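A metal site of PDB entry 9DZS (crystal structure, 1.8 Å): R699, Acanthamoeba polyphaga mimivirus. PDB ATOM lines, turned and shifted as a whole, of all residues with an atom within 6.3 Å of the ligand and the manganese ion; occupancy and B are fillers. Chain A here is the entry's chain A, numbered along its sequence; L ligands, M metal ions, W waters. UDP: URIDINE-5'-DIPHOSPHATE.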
ATOM      1  N   GLY A  17     -17.000 -21.868 -13.727  1.00  0.00           N
ATOM      2  CA  GLY A  17     -17.652 -21.175 -14.837  1.00  0.00           C
ATOM      3  C   GLY A  17     -18.969 -21.851 -15.156  1.00  0.00           C
ATOM      4  O   GLY A  17     -19.030 -23.092 -15.314  1.00  0.00           O
ATOM      5  N   ILE A  18     -20.020 -21.038 -15.302  1.00  0.00           N
ATOM      6  CA  ILE A  18     -21.336 -21.570 -15.631  1.00  0.00           C
ATOM      7  C   ILE A  18     -21.389 -21.870 -17.130  1.00  0.00           C
ATOM      8  O   ILE A  18     -21.220 -20.976 -17.959  1.00  0.00           O
ATOM      9  CB  ILE A  18     -22.447 -20.587 -15.222  1.00  0.00           C
ATOM     10  CG1 ILE A  18     -22.336 -20.071 -13.740  1.00  0.00           C
ATOM     11  CG2 ILE A  18     -23.820 -21.204 -15.548  1.00  0.00           C
ATOM     12  CD1 ILE A  18     -22.227 -21.146 -12.666  1.00  0.00           C
ATOM     13  N   GLY A  19     -21.591 -23.142 -17.464  1.00  0.00           N
ATOM     14  CA  GLY A  19     -21.710 -23.570 -18.856  1.00  0.00           C
ATOM     15  C   GLY A  19     -22.740 -24.689 -18.982  1.00  0.00           C
ATOM     16  O   GLY A  19     -22.396 -25.860 -19.170  1.00  0.00           O
ATOM     17  N   ILE A  20     -24.015 -24.286 -18.840  1.00  0.00           N
ATOM     18  CA  ILE A  20     -25.151 -25.189 -18.880  1.00  0.00           C
ATOM     19  C   ILE A  20     -25.560 -25.338 -20.345  1.00  0.00           C
ATOM     20  O   ILE A  20     -26.156 -24.426 -20.925  1.00  0.00           O
ATOM     21  CB  ILE A  20     -26.322 -24.628 -18.054  1.00  0.00           C
ATOM     22  CG1 ILE A  20     -25.916 -24.371 -16.573  1.00  0.00           C
ATOM     23  CG2 ILE A  20     -27.528 -25.572 -18.154  1.00  0.00           C
ATOM     24  CD1 ILE A  20     -26.812 -23.350 -15.843  1.00  0.00           C
ATOM     25  N   SER A  21     -25.280 -26.530 -20.896  1.00  0.00           N
ATOM     26  CA  SER A  21     -25.547 -26.835 -22.288  1.00  0.00           C
ATOM     27  C   SER A  21     -25.292 -28.336 -22.485  1.00  0.00           C
ATOM     28  O   SER A  21     -24.379 -28.896 -21.880  1.00  0.00           O
ATOM     29  CB  SER A  21     -24.600 -26.067 -23.186  1.00  0.00           C
ATOM     30  OG  SER A  21     -25.084 -26.128 -24.532  1.00  0.00           O
ATOM     31  N   VAL A  45     -19.657 -25.579 -14.608  1.00  0.00           N
ATOM     32  CA  VAL A  45     -20.867 -25.923 -13.872  1.00  0.00           C
ATOM     33  C   VAL A  45     -22.000 -26.163 -14.862  1.00  0.00           C
ATOM     34  O   VAL A  45     -22.271 -25.337 -15.716  1.00  0.00           O
ATOM     35  CB  VAL A  45     -21.220 -24.762 -12.928  1.00  0.00           C
ATOM     36  CG1 VAL A  45     -22.630 -24.930 -12.334  1.00  0.00           C
ATOM     37  CG2 VAL A  45     -20.173 -24.633 -11.812  1.00  0.00           C
ATOM     38  N   TRP A  51     -30.255 -26.009 -20.869  1.00  0.00           N
ATOM     39  CA  TRP A  51     -30.515 -24.698 -20.322  1.00  0.00           C
ATOM     40  C   TRP A  51     -32.021 -24.455 -20.156  1.00  0.00           C
ATOM     41  O   TRP A  51     -32.793 -24.675 -21.083  1.00  0.00           O
ATOM     42  CB  TRP A  51     -29.889 -23.623 -21.223  1.00  0.00           C
ATOM     43  CG  TRP A  51     -30.259 -22.200 -20.907  1.00  0.00           C
ATOM     44  CD1 TRP A  51     -31.130 -21.438 -21.620  1.00  0.00           C
ATOM     45  CD2 TRP A  51     -29.721 -21.344 -19.870  1.00  0.00           C
ATOM     46  NE1 TRP A  51     -31.223 -20.180 -21.075  1.00  0.00           N
ATOM     47  CE2 TRP A  51     -30.341 -20.086 -20.022  1.00  0.00           C
ATOM     48  CE3 TRP A  51     -28.784 -21.507 -18.850  1.00  0.00           C
ATOM     49  CZ2 TRP A  51     -30.048 -19.007 -19.183  1.00  0.00           C
ATOM     50  CZ3 TRP A  51     -28.470 -20.428 -18.048  1.00  0.00           C
ATOM     51  CH2 TRP A  51     -29.097 -19.191 -18.207  1.00  0.00           C
ATOM     52  N   GLY A  54     -34.054 -19.220 -19.235  1.00  0.00           N
ATOM     53  CA  GLY A  54     -34.905 -18.235 -19.902  1.00  0.00           C
ATOM     54  C   GLY A  54     -34.202 -17.644 -21.124  1.00  0.00           C
ATOM     55  O   GLY A  54     -32.999 -17.793 -21.267  1.00  0.00           O
ATOM     56  N   LEU A  56     -32.579 -14.945 -22.279  1.00  0.00           N
ATOM     57  CA  LEU A  56     -31.940 -13.819 -21.612  1.00  0.00           C
ATOM     58  C   LEU A  56     -31.984 -12.554 -22.478  1.00  0.00           C
ATOM     59  O   LEU A  56     -32.089 -11.443 -21.961  1.00  0.00           O
ATOM     60  CB  LEU A  56     -30.530 -14.171 -21.144  1.00  0.00           C
ATOM     61  CG  LEU A  56     -30.407 -15.155 -19.971  1.00  0.00           C
ATOM     62  CD1 LEU A  56     -28.968 -15.259 -19.526  1.00  0.00           C
ATOM     63  CD2 LEU A  56     -31.299 -14.806 -18.786  1.00  0.00           C
ATOM     64  N   LYS A  65     -28.732 -20.735 -13.106  1.00  0.00           N
ATOM     65  CA  LYS A  65     -27.299 -20.660 -12.855  1.00  0.00           C
ATOM     66  C   LYS A  65     -27.002 -20.854 -11.362  1.00  0.00           C
ATOM     67  O   LYS A  65     -26.048 -21.526 -10.974  1.00  0.00           O
ATOM     68  CB  LYS A  65     -26.714 -19.310 -13.310  1.00  0.00           C
ATOM     69  CG  LYS A  65     -26.895 -19.004 -14.804  1.00  0.00           C
ATOM     70  CD  LYS A  65     -26.044 -17.798 -15.213  1.00  0.00           C
ATOM     71  CE  LYS A  65     -26.458 -16.510 -14.614  1.00  0.00           C
ATOM     72  NZ  LYS A  65     -25.419 -15.492 -14.788  1.00  0.00           N
ATOM     73  N   CYS A  85     -18.358 -17.391 -12.441  1.00  0.00           N
ATOM     74  CA  CYS A  85     -18.412 -16.457 -13.561  1.00  0.00           C
ATOM     75  C   CYS A  85     -19.166 -17.062 -14.750  1.00  0.00           C
ATOM     76  O   CYS A  85     -19.165 -18.273 -14.963  1.00  0.00           O
ATOM     77  CB  CYS A  85     -17.004 -15.994 -13.973  1.00  0.00           C
ATOM     78  SG  CYS A  85     -15.929 -17.358 -14.492  1.00  0.00           S
ATOM     79  N   ASP A  86     -19.692 -16.144 -15.556  1.00  0.00           N
ATOM     80  CA  ASP A  86     -20.157 -16.445 -16.901  1.00  0.00           C
ATOM     81  C   ASP A  86     -19.019 -17.053 -17.700  1.00  0.00           C
ATOM     82  O   ASP A  86     -17.847 -16.776 -17.402  1.00  0.00           O
ATOM     83  CB  ASP A  86     -20.587 -15.162 -17.603  1.00  0.00           C
ATOM     84  CG  ASP A  86     -21.924 -14.584 -17.168  1.00  0.00           C
ATOM     85  OD1 ASP A  86     -22.514 -15.090 -16.176  1.00  0.00           O
ATOM     86  OD2 ASP A  86     -22.352 -13.580 -17.778  1.00  0.00           O
ATOM     87  N   THR A  87     -19.355 -17.823 -18.759  1.00  0.00           N
ATOM     88  CA  THR A  87     -18.295 -18.378 -19.621  1.00  0.00           C
ATOM     89  C   THR A  87     -18.523 -18.031 -21.096  1.00  0.00           C
ATOM     90  O   THR A  87     -17.569 -18.139 -21.882  1.00  0.00           O
ATOM     91  CB  THR A  87     -18.111 -19.885 -19.486  1.00  0.00           C
ATOM     92  OG1 THR A  87     -19.344 -20.481 -19.898  1.00  0.00           O
ATOM     93  CG2 THR A  87     -17.787 -20.267 -18.035  1.00  0.00           C
ATOM     94  N   TYR A  88     -19.754 -17.676 -21.480  1.00  0.00           N
ATOM     95  CA  TYR A  88     -19.996 -17.573 -22.915  1.00  0.00           C
ATOM     96  C   TYR A  88     -19.295 -16.359 -23.514  1.00  0.00           C
ATOM     97  O   TYR A  88     -18.915 -16.366 -24.712  1.00  0.00           O
ATOM     98  CB  TYR A  88     -21.502 -17.548 -23.216  1.00  0.00           C
ATOM     99  CG  TYR A  88     -22.141 -18.933 -23.154  1.00  0.00           C
ATOM    100  CD1 TYR A  88     -21.517 -20.000 -22.480  1.00  0.00           C
ATOM    101  CD2 TYR A  88     -23.364 -19.164 -23.775  1.00  0.00           C
ATOM    102  CE1 TYR A  88     -22.131 -21.253 -22.404  1.00  0.00           C
ATOM    103  CE2 TYR A  88     -23.965 -20.418 -23.729  1.00  0.00           C
ATOM    104  CZ  TYR A  88     -23.346 -21.449 -23.034  1.00  0.00           C
ATOM    105  OH  TYR A  88     -23.957 -22.684 -23.032  1.00  0.00           O
ATOM    106  N   ASP A  89     -19.124 -15.340 -22.687  1.00  0.00           N
ATOM    107  CA  ASP A  89     -18.681 -14.009 -23.091  1.00  0.00           C
ATOM    108  C   ASP A  89     -17.628 -13.476 -22.115  1.00  0.00           C
ATOM    109  O   ASP A  89     -17.584 -12.287 -21.803  1.00  0.00           O
ATOM    110  CB  ASP A  89     -19.856 -13.057 -23.103  1.00  0.00           C
ATOM    111  CG  ASP A  89     -20.599 -12.869 -21.777  1.00  0.00           C
ATOM    112  OD1 ASP A  89     -20.351 -13.646 -20.847  1.00  0.00           O
ATOM    113  OD2 ASP A  89     -21.384 -11.926 -21.691  1.00  0.00           O
ATOM    114  N   LEU A  90     -16.784 -14.370 -21.603  1.00  0.00           N
ATOM    115  CA  LEU A  90     -15.837 -13.984 -20.567  1.00  0.00           C
ATOM    116  C   LEU A  90     -14.565 -14.844 -20.636  1.00  0.00           C
ATOM    117  O   LEU A  90     -14.626 -16.053 -20.844  1.00  0.00           O
ATOM    118  CB  LEU A  90     -16.557 -14.153 -19.208  1.00  0.00           C
ATOM    119  CG  LEU A  90     -15.776 -13.721 -17.955  1.00  0.00           C
ATOM    120  CD1 LEU A  90     -16.787 -13.364 -16.817  1.00  0.00           C
ATOM    121  CD2 LEU A  90     -14.850 -14.816 -17.421  1.00  0.00           C
ATOM    122  N   TRP A 121     -29.643  -2.328 -13.111  1.00  0.00           N
ATOM    123  CA  TRP A 121     -30.685  -3.107 -13.759  1.00  0.00           C
ATOM    124  C   TRP A 121     -30.850  -4.445 -13.050  1.00  0.00           C
ATOM    125  O   TRP A 121     -29.919  -4.910 -12.404  1.00  0.00           O
ATOM    126  CB  TRP A 121     -30.364  -3.314 -15.248  1.00  0.00           C
ATOM    127  CG  TRP A 121     -29.226  -4.279 -15.460  1.00  0.00           C
ATOM    128  CD1 TRP A 121     -27.899  -3.966 -15.400  1.00  0.00           C
ATOM    129  CD2 TRP A 121     -29.300  -5.690 -15.724  1.00  0.00           C
ATOM    130  NE1 TRP A 121     -27.135  -5.083 -15.615  1.00  0.00           N
ATOM    131  CE2 TRP A 121     -27.961  -6.154 -15.848  1.00  0.00           C
ATOM    132  CE3 TRP A 121     -30.344  -6.611 -15.901  1.00  0.00           C
ATOM    133  CZ2 TRP A 121     -27.641  -7.487 -16.123  1.00  0.00           C
ATOM    134  CZ3 TRP A 121     -30.032  -7.926 -16.204  1.00  0.00           C
ATOM    135  CH2 TRP A 121     -28.699  -8.355 -16.306  1.00  0.00           C
ATOM    136  N   ASN A 141     -22.797  -6.113 -11.097  1.00  0.00           N
ATOM    137  CA  ASN A 141     -23.014  -7.003 -12.235  1.00  0.00           C
ATOM    138  C   ASN A 141     -22.779  -8.435 -11.743  1.00  0.00           C
ATOM    139  O   ASN A 141     -21.749  -8.733 -11.138  1.00  0.00           O
ATOM    140  CB  ASN A 141     -22.103  -6.661 -13.421  1.00  0.00           C
ATOM    141  CG  ASN A 141     -22.323  -7.689 -14.518  1.00  0.00           C
ATOM    142  OD1 ASN A 141     -21.726  -8.771 -14.471  1.00  0.00           O
ATOM    143  ND2 ASN A 141     -23.162  -7.386 -15.500  1.00  0.00           N
ATOM    144  N   GLY A 143     -22.373 -11.292 -13.249  1.00  0.00           N
ATOM    145  CA  GLY A 143     -21.661 -12.132 -14.209  1.00  0.00           C
ATOM    146  C   GLY A 143     -20.272 -12.619 -13.722  1.00  0.00           C
ATOM    147  O   GLY A 143     -19.699 -13.538 -14.299  1.00  0.00           O
ATOM    148  N   HIS A 219     -15.110  -9.418 -19.290  1.00  0.00           N
ATOM    149  CA  HIS A 219     -16.488  -9.830 -19.459  1.00  0.00           C
ATOM    150  C   HIS A 219     -17.142  -8.953 -20.530  1.00  0.00           C
ATOM    151  O   HIS A 219     -17.418  -7.774 -20.295  1.00  0.00           O
ATOM    152  CB  HIS A 219     -17.222  -9.774 -18.109  1.00  0.00           C
ATOM    153  CG  HIS A 219     -18.614 -10.273 -18.225  1.00  0.00           C
ATOM    154  ND1 HIS A 219     -19.556 -10.001 -17.258  1.00  0.00           N
ATOM    155  CD2 HIS A 219     -19.223 -11.033 -19.155  1.00  0.00           C
ATOM    156  CE1 HIS A 219     -20.710 -10.572 -17.582  1.00  0.00           C
ATOM    157  NE2 HIS A 219     -20.521 -11.220 -18.735  1.00  0.00           N
ATOM    158  N   GLY A 220     -17.411  -9.546 -21.697  1.00  0.00           N
ATOM    159  CA  GLY A 220     -18.114  -8.813 -22.764  1.00  0.00           C
ATOM    160  C   GLY A 220     -19.626  -8.874 -22.542  1.00  0.00           C
ATOM    161  O   GLY A 220     -20.344  -9.492 -23.322  1.00  0.00           O
ATOM    162  N   ASN A 221     -20.099  -8.266 -21.437  1.00  0.00           N
ATOM    163  CA  ASN A 221     -21.487  -8.418 -21.018  1.00  0.00           C
ATOM    164  C   ASN A 221     -22.385  -7.708 -22.047  1.00  0.00           C
ATOM    165  O   ASN A 221     -21.994  -6.691 -22.647  1.00  0.00           O
ATOM    166  CB  ASN A 221     -21.720  -7.889 -19.597  1.00  0.00           C
ATOM    167  CG  ASN A 221     -21.368  -6.406 -19.433  1.00  0.00           C
ATOM    168  OD1 ASN A 221     -20.268  -5.984 -19.815  1.00  0.00           O
ATOM    169  ND2 ASN A 221     -22.263  -5.612 -18.832  1.00  0.00           N
ATOM    170  N   GLY A 222     -23.606  -8.223 -22.209  1.00  0.00           N
ATOM    171  CA  GLY A 222     -24.541  -7.641 -23.176  1.00  0.00           C
ATOM    172  C   GLY A 222     -23.916  -7.563 -24.575  1.00  0.00           C
ATOM    173  O   GLY A 222     -23.255  -8.497 -25.032  1.00  0.00           O
ATOM    174  N   PRO A 223     -24.134  -6.453 -25.305  1.00  0.00           N
ATOM    175  CA  PRO A 223     -23.570  -6.235 -26.633  1.00  0.00           C
ATOM    176  C   PRO A 223     -22.052  -6.145 -26.667  1.00  0.00           C
ATOM    177  O   PRO A 223     -21.467  -6.191 -27.747  1.00  0.00           O
ATOM    178  CB  PRO A 223     -24.171  -4.847 -27.038  1.00  0.00           C
ATOM    179  CG  PRO A 223     -25.412  -4.716 -26.172  1.00  0.00           C
ATOM    180  CD  PRO A 223     -25.005  -5.344 -24.860  1.00  0.00           C
ATOM    181  N   LYS A 225     -20.080  -8.430 -26.199  1.00  0.00           N
ATOM    182  CA  LYS A 225     -19.544  -9.643 -26.803  1.00  0.00           C
ATOM    183  C   LYS A 225     -18.713  -9.278 -28.038  1.00  0.00           C
ATOM    184  O   LYS A 225     -17.657  -9.871 -28.275  1.00  0.00           O
ATOM    185  CB  LYS A 225     -20.644 -10.657 -27.158  1.00  0.00           C
ATOM    186  CG  LYS A 225     -21.323 -11.226 -25.895  1.00  0.00           C
ATOM    187  CD  LYS A 225     -22.726 -11.743 -26.053  1.00  0.00           C
ATOM    188  CE  LYS A 225     -23.298 -12.128 -24.685  1.00  0.00           C
ATOM    189  NZ  LYS A 225     -23.177 -11.035 -23.678  1.00  0.00           N
HETATM  190  N1  UDP L   1     -25.506 -19.654 -19.956  1.00  0.00           N
HETATM  191  C2  UDP L   1     -25.365 -21.020 -19.991  1.00  0.00           C
HETATM  192  N3  UDP L   1     -26.133 -21.685 -20.915  1.00  0.00           N
HETATM  193  C4  UDP L   1     -26.954 -21.099 -21.875  1.00  0.00           C
HETATM  194  C5  UDP L   1     -27.057 -19.671 -21.785  1.00  0.00           C
HETATM  195  C6  UDP L   1     -26.311 -19.009 -20.871  1.00  0.00           C
HETATM  196  O2  UDP L   1     -24.618 -21.596 -19.210  1.00  0.00           O
HETATM  197  O4  UDP L   1     -27.568 -21.810 -22.677  1.00  0.00           O
HETATM  198  C1' UDP L   1     -24.647 -18.942 -18.977  1.00  0.00           C
HETATM  199  C2' UDP L   1     -23.270 -18.560 -19.585  1.00  0.00           C
HETATM  200  O2' UDP L   1     -22.257 -18.611 -18.597  1.00  0.00           O
HETATM  201  C3' UDP L   1     -23.519 -17.098 -19.974  1.00  0.00           C
HETATM  202  C4' UDP L   1     -24.349 -16.614 -18.777  1.00  0.00           C
HETATM  203  O4' UDP L   1     -25.269 -17.721 -18.609  1.00  0.00           O
HETATM  204  O3' UDP L   1     -22.295 -16.403 -20.117  1.00  0.00           O
HETATM  205  C5' UDP L   1     -25.145 -15.327 -18.876  1.00  0.00           C
HETATM  206  O5' UDP L   1     -25.579 -15.099 -20.255  1.00  0.00           O
HETATM  207  PA  UDP L   1     -24.895 -13.884 -21.027  1.00  0.00           P
HETATM  208  O1A UDP L   1     -25.301 -13.886 -22.457  1.00  0.00           O
HETATM  209  O2A UDP L   1     -23.436 -13.867 -20.725  1.00  0.00           O
HETATM  210  O3A UDP L   1     -25.556 -12.627 -20.280  1.00  0.00           O
HETATM  211  PB  UDP L   1     -25.026 -11.122 -20.188  1.00  0.00           P
HETATM  212  O1B UDP L   1     -24.973 -10.592 -21.602  1.00  0.00           O
HETATM  213  O2B UDP L   1     -23.705 -11.137 -19.446  1.00  0.00           O
HETATM  214  O3B UDP L   1     -26.110 -10.428 -19.306  1.00  0.00           O
HETATM  215 MN    MN M   1     -22.099 -12.509 -19.658  1.00  0.00          MN
HETATM  216  O   HOH W   1     -28.145 -24.450 -23.839  1.00  0.00           O
HETATM  217  O   HOH W   2     -26.901 -10.539 -23.416  1.00  0.00           O
HETATM  218  O   HOH W   3     -25.900 -23.251 -24.768  1.00  0.00           O
HETATM  219  O   HOH W   4     -27.348 -12.999 -23.957  1.00  0.00           O
HETATM  220  O   HOH W   5     -24.369 -15.677 -24.123  1.00  0.00           O
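O2B of the ligand binds the manganese ion, 2.1 Å away.
The manganese ion is bound by OD2 of Asp 86 (2.2 Å).
O2A of the ligand binds the manganese ion, 2.2 Å away.
The manganese ion is bound by OD2 of Asp 89, 2.2 Å away.
NE2 of His 219 is bound to the manganese ion, 2.2 Å away.
The side-chain carboxylate (OD1) of Asp 89 binds the manganese ion, 2.4 Å away.
The backbone NH of Gly 222 is in hydrogen-bond range of an oxygen (O1B) of the ligand.
NZ of Lys 225 lies within salt-bridge range of O1B of the ligand (2.8 Å).
OH of Tyr 88 is in hydrogen-bond range of N3 of the ligand, at 3.2 Å.
The backbone NH of Thr 87 is in hydrogen-bond range of an oxygen (O2') of the ligand (3.0 Å).
O2' of the ligand is in hydrogen-bond range of O of Ile 18 (2.7 Å).
O of Ile 20 is in hydrogen-bond range of N3 of the ligand (2.7 Å).
An oxygen (O2) of the ligand lies within hydrogen-bond range of the backbone NH of Ile 20.
The backbone NH (N) of Tyr 88 lies within hydrogen-bond range of an oxygen (O3') of the ligand (3.2 Å).
Three residues have an atom within 4 Å of the manganese ion: Asp 86, Asp 89 and His 219.
Water W3 lies within hydrogen-bond range of OH of Tyr 88 (2.7 Å), OG of Ser 21 (3.0 Å) and O4 of the ligand (3.0 Å).
The backbone NH of Gly 19 lies within hydrogen-bond range of the backbone carbonyl oxygen of Val 45, at 2.9 Å.
OD1 of Asn 221 sits close to O of His 219.
The side-chain amino group (NZ) of Lys 225 lies close to the side-chain carboxylate (OD2) of Asp 89, at 2.8 Å.
The side-chain amino group of Lys 225 is in hydrogen-bond range of the backbone carbonyl oxygen of Gly 222 (2.9 Å).
N of Asp 86 sits at hydrogen-bond distance from O of Gly 143 (2.9 Å).
NE1 of Trp 51 sits at hydrogen-bond distance from O of Gly 54, 3.0 Å away.
The backbone NH (N) of Lys 225 lies within hydrogen-bond range of the backbone carbonyl oxygen (O) of Gly 220, at 3.1 Å.
The backbone carbonyl oxygen (O) of Asp 89 lies within hydrogen-bond range of the backbone NH (N) of Gly 220 (2.7 Å).
Residues that only touch the ligand: Gly 19 (3.5 Å), Trp 51 (3.2 Å), Leu 56 (3.5 Å), Lys 65 (3.5 Å) and Asn 221 (3.8 Å).
Hydrophobic or aromatic side chains that line the ligand: Ile 18, Ile 20, Trp 51, Leu 56, Tyr 88 and His 219.
14 residues have an atom within 4 Å of the ligand: Ile 18, Gly 19, Ile 20, Trp 51, Leu 56, Lys 65, Asp 86, Thr 87, Tyr 88, Asp 89, His 219, Asn 221, Gly 222 and Lys 225.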
